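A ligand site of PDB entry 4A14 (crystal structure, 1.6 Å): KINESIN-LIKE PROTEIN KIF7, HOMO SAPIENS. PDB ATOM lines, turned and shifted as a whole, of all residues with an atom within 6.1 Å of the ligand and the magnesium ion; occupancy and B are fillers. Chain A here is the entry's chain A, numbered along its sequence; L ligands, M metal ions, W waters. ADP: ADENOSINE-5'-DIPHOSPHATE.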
ATOM      1  N   ARG A  18     -14.667 -17.315   4.525  1.00  0.00           N
ATOM      2  CA  ARG A  18     -15.417 -16.078   4.532  1.00  0.00           C
ATOM      3  C   ARG A  18     -16.043 -15.836   3.175  1.00  0.00           C
ATOM      4  O   ARG A  18     -15.361 -15.686   2.172  1.00  0.00           O
ATOM      5  CB  ARG A  18     -14.531 -14.888   4.927  1.00  0.00           C
ATOM      6  CG  ARG A  18     -15.442 -13.627   5.071  1.00  0.00           C
ATOM      7  CD  ARG A  18     -14.652 -12.342   5.321  1.00  0.00           C
ATOM      8  NE  ARG A  18     -15.573 -11.299   5.799  1.00  0.00           N
ATOM      9  CZ  ARG A  18     -15.179 -10.077   6.142  1.00  0.00           C
ATOM     10  NH1 ARG A  18     -13.896  -9.708   5.994  1.00  0.00           N
ATOM     11  NH2 ARG A  18     -16.083  -9.241   6.625  1.00  0.00           N
ATOM     12  N   VAL A  19     -17.380 -15.828   3.132  1.00  0.00           N
ATOM     13  CA  VAL A  19     -18.052 -15.523   1.899  1.00  0.00           C
ATOM     14  C   VAL A  19     -18.476 -14.066   1.862  1.00  0.00           C
ATOM     15  O   VAL A  19     -19.151 -13.602   2.761  1.00  0.00           O
ATOM     16  CB  VAL A  19     -19.318 -16.402   1.760  1.00  0.00           C
ATOM     17  CG1 VAL A  19     -19.978 -16.170   0.393  1.00  0.00           C
ATOM     18  CG2 VAL A  19     -18.972 -17.869   1.973  1.00  0.00           C
ATOM     19  N   ARG A  20     -18.022 -13.329   0.848  1.00  0.00           N
ATOM     20  CA  ARG A  20     -18.404 -11.919   0.735  1.00  0.00           C
ATOM     21  C   ARG A  20     -19.786 -11.764   0.070  1.00  0.00           C
ATOM     22  O   ARG A  20     -20.297 -12.719  -0.528  1.00  0.00           O
ATOM     23  CB  ARG A  20     -17.348 -11.119  -0.015  1.00  0.00           C
ATOM     24  CG  ARG A  20     -17.084 -11.543  -1.448  1.00  0.00           C
ATOM     25  CD  ARG A  20     -16.624 -10.286  -2.209  1.00  0.00           C
ATOM     26  NE  ARG A  20     -16.094 -10.568  -3.538  1.00  0.00           N
ATOM     27  CZ  ARG A  20     -16.869 -10.762  -4.618  1.00  0.00           C
ATOM     28  NH1 ARG A  20     -18.203 -10.771  -4.529  1.00  0.00           N
ATOM     29  NH2 ARG A  20     -16.295 -10.966  -5.800  1.00  0.00           N
ATOM     30  N   PRO A  21     -20.380 -10.566   0.167  1.00  0.00           N
ATOM     31  CA  PRO A  21     -21.588 -10.321  -0.650  1.00  0.00           C
ATOM     32  C   PRO A  21     -21.283 -10.319  -2.144  1.00  0.00           C
ATOM     33  O   PRO A  21     -20.166 -10.149  -2.568  1.00  0.00           O
ATOM     34  CB  PRO A  21     -22.050  -8.929  -0.204  1.00  0.00           C
ATOM     35  CG  PRO A  21     -20.926  -8.344   0.535  1.00  0.00           C
ATOM     36  CD  PRO A  21     -20.009  -9.399   0.979  1.00  0.00           C
ATOM     37  N   LEU A  23     -21.157  -8.376  -5.310  1.00  0.00           N
ATOM     38  CA  LEU A  23     -20.903  -6.940  -5.482  1.00  0.00           C
ATOM     39  C   LEU A  23     -21.896  -6.329  -6.473  1.00  0.00           C
ATOM     40  O   LEU A  23     -22.397  -7.024  -7.345  1.00  0.00           O
ATOM     41  CB  LEU A  23     -19.469  -6.706  -5.974  1.00  0.00           C
ATOM     42  CG  LEU A  23     -18.418  -7.261  -4.995  1.00  0.00           C
ATOM     43  CD1 LEU A  23     -17.046  -7.308  -5.643  1.00  0.00           C
ATOM     44  CD2 LEU A  23     -18.390  -6.411  -3.751  1.00  0.00           C
ATOM     45  N   GLU A  60     -22.020 -13.440   4.425  1.00  0.00           N
ATOM     46  CA  GLU A  60     -21.833 -12.096   3.876  1.00  0.00           C
ATOM     47  C   GLU A  60     -22.173 -11.019   4.889  1.00  0.00           C
ATOM     48  O   GLU A  60     -21.712  -9.888   4.770  1.00  0.00           O
ATOM     49  CB  GLU A  60     -22.641 -11.909   2.595  1.00  0.00           C
ATOM     50  CG  GLU A  60     -24.157 -11.968   2.844  1.00  0.00           C
ATOM     51  CD  GLU A  60     -24.937 -11.750   1.566  1.00  0.00           C
ATOM     52  OE1 GLU A  60     -24.398 -12.041   0.483  1.00  0.00           O
ATOM     53  OE2 GLU A  60     -26.100 -11.296   1.645  1.00  0.00           O
ATOM     54  N   ALA A  62     -21.373 -11.204   8.120  1.00  0.00           N
ATOM     55  CA  ALA A  62     -20.420 -11.090   9.210  1.00  0.00           C
ATOM     56  C   ALA A  62     -19.504  -9.891   8.971  1.00  0.00           C
ATOM     57  O   ALA A  62     -18.773  -9.845   7.995  1.00  0.00           O
ATOM     58  CB  ALA A  62     -19.579 -12.339   9.309  1.00  0.00           C
ATOM     59  N   GLN A  64     -16.460  -6.990  10.080  1.00  0.00           N
ATOM     60  CA  GLN A  64     -15.034  -7.106  10.367  1.00  0.00           C
ATOM     61  C   GLN A  64     -14.769  -7.493  11.814  1.00  0.00           C
ATOM     62  O   GLN A  64     -13.877  -8.285  12.085  1.00  0.00           O
ATOM     63  CB  GLN A  64     -14.333  -5.792  10.040  1.00  0.00           C
ATOM     64  CG  GLN A  64     -14.472  -5.359   8.600  1.00  0.00           C
ATOM     65  CD  GLN A  64     -13.548  -6.131   7.675  1.00  0.00           C
ATOM     66  OE1 GLN A  64     -13.647  -7.370   7.564  1.00  0.00           O
ATOM     67  NE2 GLN A  64     -12.646  -5.415   7.002  1.00  0.00           N
ATOM     68  N   GLY A  91      -7.326 -16.871  -1.597  1.00  0.00           N
ATOM     69  CA  GLY A  91      -8.478 -16.999  -2.508  1.00  0.00           C
ATOM     70  C   GLY A  91      -8.258 -16.234  -3.805  1.00  0.00           C
ATOM     71  O   GLY A  91      -7.249 -15.535  -3.957  1.00  0.00           O
ATOM     72  N   GLN A  92      -9.211 -16.321  -4.724  1.00  0.00           N
ATOM     73  CA  GLN A  92      -9.010 -15.666  -6.018  1.00  0.00           C
ATOM     74  C   GLN A  92      -8.967 -14.141  -5.878  1.00  0.00           C
ATOM     75  O   GLN A  92      -9.499 -13.540  -4.938  1.00  0.00           O
ATOM     76  CB  GLN A  92     -10.086 -16.100  -7.023  1.00  0.00           C
ATOM     77  CG  GLN A  92     -11.385 -15.398  -6.805  1.00  0.00           C
ATOM     78  CD  GLN A  92     -12.453 -15.772  -7.829  1.00  0.00           C
ATOM     79  OE1 GLN A  92     -13.481 -16.282  -7.466  1.00  0.00           O
ATOM     80  NE2 GLN A  92     -12.218 -15.487  -9.116  1.00  0.00           N
ATOM     81  N   THR A  93      -8.325 -13.486  -6.839  1.00  0.00           N
ATOM     82  CA  THR A  93      -8.407 -12.039  -6.895  1.00  0.00           C
ATOM     83  C   THR A  93      -9.876 -11.591  -6.893  1.00  0.00           C
ATOM     84  O   THR A  93     -10.692 -12.124  -7.665  1.00  0.00           O
ATOM     85  CB  THR A  93      -7.613 -11.518  -8.126  1.00  0.00           C
ATOM     86  OG1 THR A  93      -6.250 -11.938  -7.978  1.00  0.00           O
ATOM     87  CG2 THR A  93      -7.638 -10.003  -8.200  1.00  0.00           C
ATOM     88  N   GLY A  94     -10.193 -10.620  -6.044  1.00  0.00           N
ATOM     89  CA  GLY A  94     -11.545 -10.077  -5.926  1.00  0.00           C
ATOM     90  C   GLY A  94     -12.388 -10.731  -4.856  1.00  0.00           C
ATOM     91  O   GLY A  94     -13.549 -10.359  -4.687  1.00  0.00           O
ATOM     92  N   SER A  95     -11.832 -11.715  -4.160  1.00  0.00           N
ATOM     93  CA  SER A  95     -12.649 -12.500  -3.215  1.00  0.00           C
ATOM     94  C   SER A  95     -12.742 -11.828  -1.838  1.00  0.00           C
ATOM     95  O   SER A  95     -13.665 -12.119  -1.072  1.00  0.00           O
ATOM     96  CB  SER A  95     -12.107 -13.921  -3.063  1.00  0.00           C
ATOM     97  OG  SER A  95     -10.786 -13.917  -2.551  1.00  0.00           O
ATOM     98  N   GLY A  96     -11.883 -10.862  -1.583  1.00  0.00           N
ATOM     99  CA  GLY A  96     -11.862 -10.145  -0.316  1.00  0.00           C
ATOM    100  C   GLY A  96     -10.693 -10.335   0.626  1.00  0.00           C
ATOM    101  O   GLY A  96     -10.786  -9.975   1.799  1.00  0.00           O
ATOM    102  N   LYS A  97      -9.607 -10.913   0.117  1.00  0.00           N
ATOM    103  CA  LYS A  97      -8.389 -11.076   0.960  1.00  0.00           C
ATOM    104  C   LYS A  97      -7.850  -9.761   1.591  1.00  0.00           C
ATOM    105  O   LYS A  97      -7.593  -9.700   2.796  1.00  0.00           O
ATOM    106  CB  LYS A  97      -7.250 -11.707   0.156  1.00  0.00           C
ATOM    107  CG  LYS A  97      -7.504 -13.079  -0.390  1.00  0.00           C
ATOM    108  CD  LYS A  97      -6.232 -13.593  -1.105  1.00  0.00           C
ATOM    109  CE  LYS A  97      -5.864 -12.696  -2.316  1.00  0.00           C
ATOM    110  NZ  LYS A  97      -6.964 -12.636  -3.379  1.00  0.00           N
ATOM    111  N   THR A  98      -7.652  -8.725   0.784  1.00  0.00           N
ATOM    112  CA  THR A  98      -7.111  -7.478   1.321  1.00  0.00           C
ATOM    113  C   THR A  98      -8.098  -6.760   2.237  1.00  0.00           C
ATOM    114  O   THR A  98      -7.723  -6.212   3.294  1.00  0.00           O
ATOM    115  CB  THR A  98      -6.663  -6.551   0.160  1.00  0.00           C
ATOM    116  OG1 THR A  98      -5.650  -7.239  -0.573  1.00  0.00           O
ATOM    117  CG2 THR A  98      -6.060  -5.240   0.692  1.00  0.00           C
ATOM    118  N   TYR A  99      -9.363  -6.752   1.831  1.00  0.00           N
ATOM    119  CA  TYR A  99     -10.393  -6.205   2.704  1.00  0.00           C
ATOM    120  C   TYR A  99     -10.385  -6.888   4.056  1.00  0.00           C
ATOM    121  O   TYR A  99     -10.458  -6.244   5.096  1.00  0.00           O
ATOM    122  CB  TYR A  99     -11.764  -6.336   2.048  1.00  0.00           C
ATOM    123  CG  TYR A  99     -12.919  -5.894   2.913  1.00  0.00           C
ATOM    124  CD1 TYR A  99     -13.215  -4.539   3.069  1.00  0.00           C
ATOM    125  CD2 TYR A  99     -13.716  -6.814   3.557  1.00  0.00           C
ATOM    126  CE1 TYR A  99     -14.292  -4.126   3.844  1.00  0.00           C
ATOM    127  CE2 TYR A  99     -14.808  -6.425   4.349  1.00  0.00           C
ATOM    128  CZ  TYR A  99     -15.087  -5.079   4.477  1.00  0.00           C
ATOM    129  OH  TYR A  99     -16.149  -4.667   5.254  1.00  0.00           O
ATOM    130  N   THR A 100     -10.293  -8.213   4.053  1.00  0.00           N
ATOM    131  CA  THR A 100     -10.247  -8.963   5.294  1.00  0.00           C
ATOM    132  C   THR A 100      -8.992  -8.695   6.137  1.00  0.00           C
ATOM    133  O   THR A 100      -9.086  -8.486   7.348  1.00  0.00           O
ATOM    134  CB  THR A 100     -10.398 -10.459   4.987  1.00  0.00           C
ATOM    135  OG1 THR A 100     -11.682 -10.661   4.416  1.00  0.00           O
ATOM    136  CG2 THR A 100     -10.267 -11.318   6.260  1.00  0.00           C
ATOM    137  N   GLU A 113     -15.010  -0.492   9.236  1.00  0.00           N
ATOM    138  CA  GLU A 113     -14.622  -1.311   8.101  1.00  0.00           C
ATOM    139  C   GLU A 113     -13.153  -1.754   8.181  1.00  0.00           C
ATOM    140  O   GLU A 113     -12.666  -2.458   7.292  1.00  0.00           O
ATOM    141  CB  GLU A 113     -14.847  -0.553   6.789  1.00  0.00           C
ATOM    142  CG  GLU A 113     -16.309  -0.260   6.474  1.00  0.00           C
ATOM    143  CD  GLU A 113     -17.146  -1.523   6.360  1.00  0.00           C
ATOM    144  OE1 GLU A 113     -17.038  -2.230   5.333  1.00  0.00           O
ATOM    145  OE2 GLU A 113     -17.914  -1.813   7.317  1.00  0.00           O
ATOM    146  N   SER A 211      -0.263  -6.273  -7.645  1.00  0.00           N
ATOM    147  CA  SER A 211      -0.297  -6.886  -6.308  1.00  0.00           C
ATOM    148  C   SER A 211      -1.177  -8.129  -6.158  1.00  0.00           C
ATOM    149  O   SER A 211      -1.069  -8.868  -5.158  1.00  0.00           O
ATOM    150  CB  SER A 211      -0.826  -5.852  -5.319  1.00  0.00           C
ATOM    151  OG  SER A 211      -2.170  -5.502  -5.611  1.00  0.00           O
ATOM    152  N   SER A 212      -2.122  -8.327  -7.071  1.00  0.00           N
ATOM    153  CA  SER A 212      -2.845  -9.599  -7.098  1.00  0.00           C
ATOM    154  C   SER A 212      -1.888 -10.766  -7.385  1.00  0.00           C
ATOM    155  O   SER A 212      -2.266 -11.917  -7.232  1.00  0.00           O
ATOM    156  CB  SER A 212      -3.981  -9.570  -8.144  1.00  0.00           C
ATOM    157  OG  SER A 212      -3.471  -9.263  -9.425  1.00  0.00           O
ATOM    158  N   ASP A 249      -1.193 -11.588   3.327  1.00  0.00           N
ATOM    159  CA  ASP A 249      -2.213 -11.371   2.293  1.00  0.00           C
ATOM    160  C   ASP A 249      -1.601 -11.991   1.070  1.00  0.00           C
ATOM    161  O   ASP A 249      -0.680 -11.456   0.458  1.00  0.00           O
ATOM    162  CB  ASP A 249      -2.431  -9.844   2.156  1.00  0.00           C
ATOM    163  CG  ASP A 249      -3.450  -9.448   1.075  1.00  0.00           C
ATOM    164  OD1 ASP A 249      -3.964 -10.306   0.318  1.00  0.00           O
ATOM    165  OD2 ASP A 249      -3.701  -8.220   0.958  1.00  0.00           O
ATOM    166  N   LEU A 250      -2.119 -13.164   0.691  1.00  0.00           N
ATOM    167  CA  LEU A 250      -1.525 -13.962  -0.370  1.00  0.00           C
ATOM    168  C   LEU A 250      -1.851 -13.476  -1.791  1.00  0.00           C
ATOM    169  O   LEU A 250      -2.816 -12.757  -2.013  1.00  0.00           O
ATOM    170  CB  LEU A 250      -1.943 -15.432  -0.264  1.00  0.00           C
ATOM    171  CG  LEU A 250      -1.449 -16.184   0.963  1.00  0.00           C
ATOM    172  CD1 LEU A 250      -2.282 -17.464   1.161  1.00  0.00           C
ATOM    173  CD2 LEU A 250       0.091 -16.471   0.840  1.00  0.00           C
ATOM    174  N   CYS A 322     -11.145 -16.918   1.426  1.00  0.00           N
ATOM    175  CA  CYS A 322     -12.137 -15.954   0.953  1.00  0.00           C
ATOM    176  C   CYS A 322     -12.704 -16.435  -0.364  1.00  0.00           C
ATOM    177  O   CYS A 322     -11.964 -16.837  -1.277  1.00  0.00           O
ATOM    178  CB  CYS A 322     -11.453 -14.593   0.747  1.00  0.00           C
ATOM    179  SG  CYS A 322     -10.794 -13.902   2.298  1.00  0.00           S
HETATM  180  PB  ADP L   1      -8.713  -9.413  -3.082  1.00  0.00           P
HETATM  181  O1B ADP L   1      -8.950 -10.857  -2.684  1.00  0.00           O
HETATM  182  O2B ADP L   1      -8.412  -9.285  -4.554  1.00  0.00           O
HETATM  183  O3B ADP L   1      -7.666  -8.688  -2.215  1.00  0.00           O
HETATM  184  PA  ADP L   1     -10.391  -7.212  -2.223  1.00  0.00           P
HETATM  185  O1A ADP L   1     -10.252  -7.076  -0.725  1.00  0.00           O
HETATM  186  O2A ADP L   1      -9.680  -6.253  -3.140  1.00  0.00           O
HETATM  187  O3A ADP L   1     -10.053  -8.636  -2.796  1.00  0.00           O
HETATM  188  O5' ADP L   1     -11.996  -7.075  -2.405  1.00  0.00           O
HETATM  189  C5' ADP L   1     -12.528  -7.012  -3.738  1.00  0.00           C
HETATM  190  C4' ADP L   1     -13.715  -6.059  -3.634  1.00  0.00           C
HETATM  191  O4' ADP L   1     -14.751  -6.603  -2.827  1.00  0.00           O
HETATM  192  C3' ADP L   1     -13.315  -4.764  -2.956  1.00  0.00           C
HETATM  193  O3' ADP L   1     -13.985  -3.688  -3.649  1.00  0.00           O
HETATM  194  C2' ADP L   1     -13.859  -4.888  -1.548  1.00  0.00           C
HETATM  195  O2' ADP L   1     -14.191  -3.648  -0.925  1.00  0.00           O
HETATM  196  C1' ADP L   1     -15.073  -5.785  -1.718  1.00  0.00           C
HETATM  197  N9  ADP L   1     -15.272  -6.697  -0.572  1.00  0.00           N
HETATM  198  C8  ADP L   1     -14.450  -7.731  -0.270  1.00  0.00           C
HETATM  199  N7  ADP L   1     -14.904  -8.375   0.819  1.00  0.00           N
HETATM  200  C5  ADP L   1     -16.046  -7.775   1.232  1.00  0.00           C
HETATM  201  C6  ADP L   1     -17.038  -7.979   2.311  1.00  0.00           C
HETATM  202  N6  ADP L   1     -16.926  -8.966   3.213  1.00  0.00           N
HETATM  203  N1  ADP L   1     -18.065  -7.098   2.379  1.00  0.00           N
HETATM  204  C2  ADP L   1     -18.206  -6.111   1.476  1.00  0.00           C
HETATM  205  N3  ADP L   1     -17.354  -5.878   0.460  1.00  0.00           N
HETATM  206  C4  ADP L   1     -16.265  -6.656   0.300  1.00  0.00           C
HETATM  207 MG    MG M   1      -5.886  -7.785  -2.558  1.00  0.00          MG
HETATM  208  O   HOH W   1     -14.371 -10.481   2.617  1.00  0.00           O
HETATM  209  O   HOH W   2     -18.352  -3.608  -0.894  1.00  0.00           O
HETATM  210  O   HOH W   3      -6.947  -6.024  -3.191  1.00  0.00           O
HETATM  211  O   HOH W   4      -4.186  -6.618  -3.004  1.00  0.00           O
HETATM  212  O   HOH W   5      -4.720  -9.460  -2.091  1.00  0.00           O
HETATM  213  O   HOH W   6      -9.964  -4.377  -4.810  1.00  0.00           O
HETATM  214  O   HOH W   7      -5.907  -8.526  -4.608  1.00  0.00           O
HETATM  215  O   HOH W   8      -9.676  -4.130  -0.518  1.00  0.00           O
HETATM  216  O   HOH W   9      -9.190  -7.211  -6.205  1.00  0.00           O
HETATM  217  O   HOH W  10     -12.114  -2.597  -0.140  1.00  0.00           O
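OG1 of Thr 100 is in hydrogen-bond range of NH1 of Arg 18, at 2.9 Å.
The backbone carbonyl oxygen (O) of Gly 94 sits at hydrogen-bond distance from the guanidinium group (NE) of Arg 20, 2.8 Å away.
NE2 of Gln 64 sits at hydrogen-bond distance from O of Tyr 99, 3.0 Å away.
The side-chain hydroxyl of Ser 95 is in hydrogen-bond range of the backbone carbonyl oxygen of Gln 92, at 2.7 Å.
The side-chain amino group of Lys 97 is in hydrogen-bond range of the backbone carbonyl oxygen of Gln 92 (3.1 Å).
NH2 of Arg 18 lies within hydrogen-bond range of O of Ala 62 (3.1 Å).
The side-chain carboxylate (OE1) of Glu 113 is in hydrogen-bond range of the side-chain hydroxyl (OH) of Tyr 99 (2.6 Å).
O of Gly 96 sits at hydrogen-bond distance from OG1 of Thr 100.
The magnesium ion is bound by an oxygen (O3B) of the ligand (2.0 Å), the side-chain hydroxyl of Thr 98 (2.1 Å), water W5 (2.1 Å), water W4 (2.1 Å), water W3 (2.2 Å) and water W7 (2.2 Å).
Water W1 lies within hydrogen-bond range of N7 of the ligand, OG1 of Thr 100 and NH1 of Arg 18.
Arg 18 touches the ligand (NH2 to N6, 3.5 Å).
CB of Arg 20 touches N7 of the ligand (3.8 Å).
Pro 21 touches the ligand (CD to N1, 3.3 Å).
CD1 of Leu 23 touches O4' of the ligand, 3.7 Å away.
O of Gln 92 touches O1B of the ligand, 3.5 Å away.
C of Thr 93 touches O2B of the ligand, 3.6 Å away.
Hydrophobic or aromatic side chains that line the ligand: Pro 21, Leu 23 and Tyr 99.
Within 4 Å of the ligand: Arg 18, Arg 20, Pro 21, Leu 23, Gln 92, Thr 93, Gly 94, Ser 95, Gly 96, Lys 97, Thr 98 and Tyr 99.
The nearest printed residue that does not touch the ligand is Asp 249 (4.8 Å).
N of Gly 94 sits at hydrogen-bond distance from O2B of the ligand, at 2.7 Å.
NZ of Lys 97 is in salt-bridge range of O1B of the ligand (2.8 Å).
The backbone NH (N) of Thr 98 lies within hydrogen-bond range of an oxygen (O1A) of the ligand.
N of Lys 97 sits at hydrogen-bond distance from O1B of the ligand.
The backbone NH (N) of Tyr 99 sits at hydrogen-bond distance from an oxygen (O1A) of the ligand (2.7 Å).
An oxygen (O1B) of the ligand lies within hydrogen-bond range of the backbone NH (N) of Ser 95, at 3.3 Å.
The backbone NH (N) of Gly 96 lies within hydrogen-bond range of an oxygen (O3A) of the ligand.
Of the 24 residues printed, 1 comes within 4 Å of the magnesium ion.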
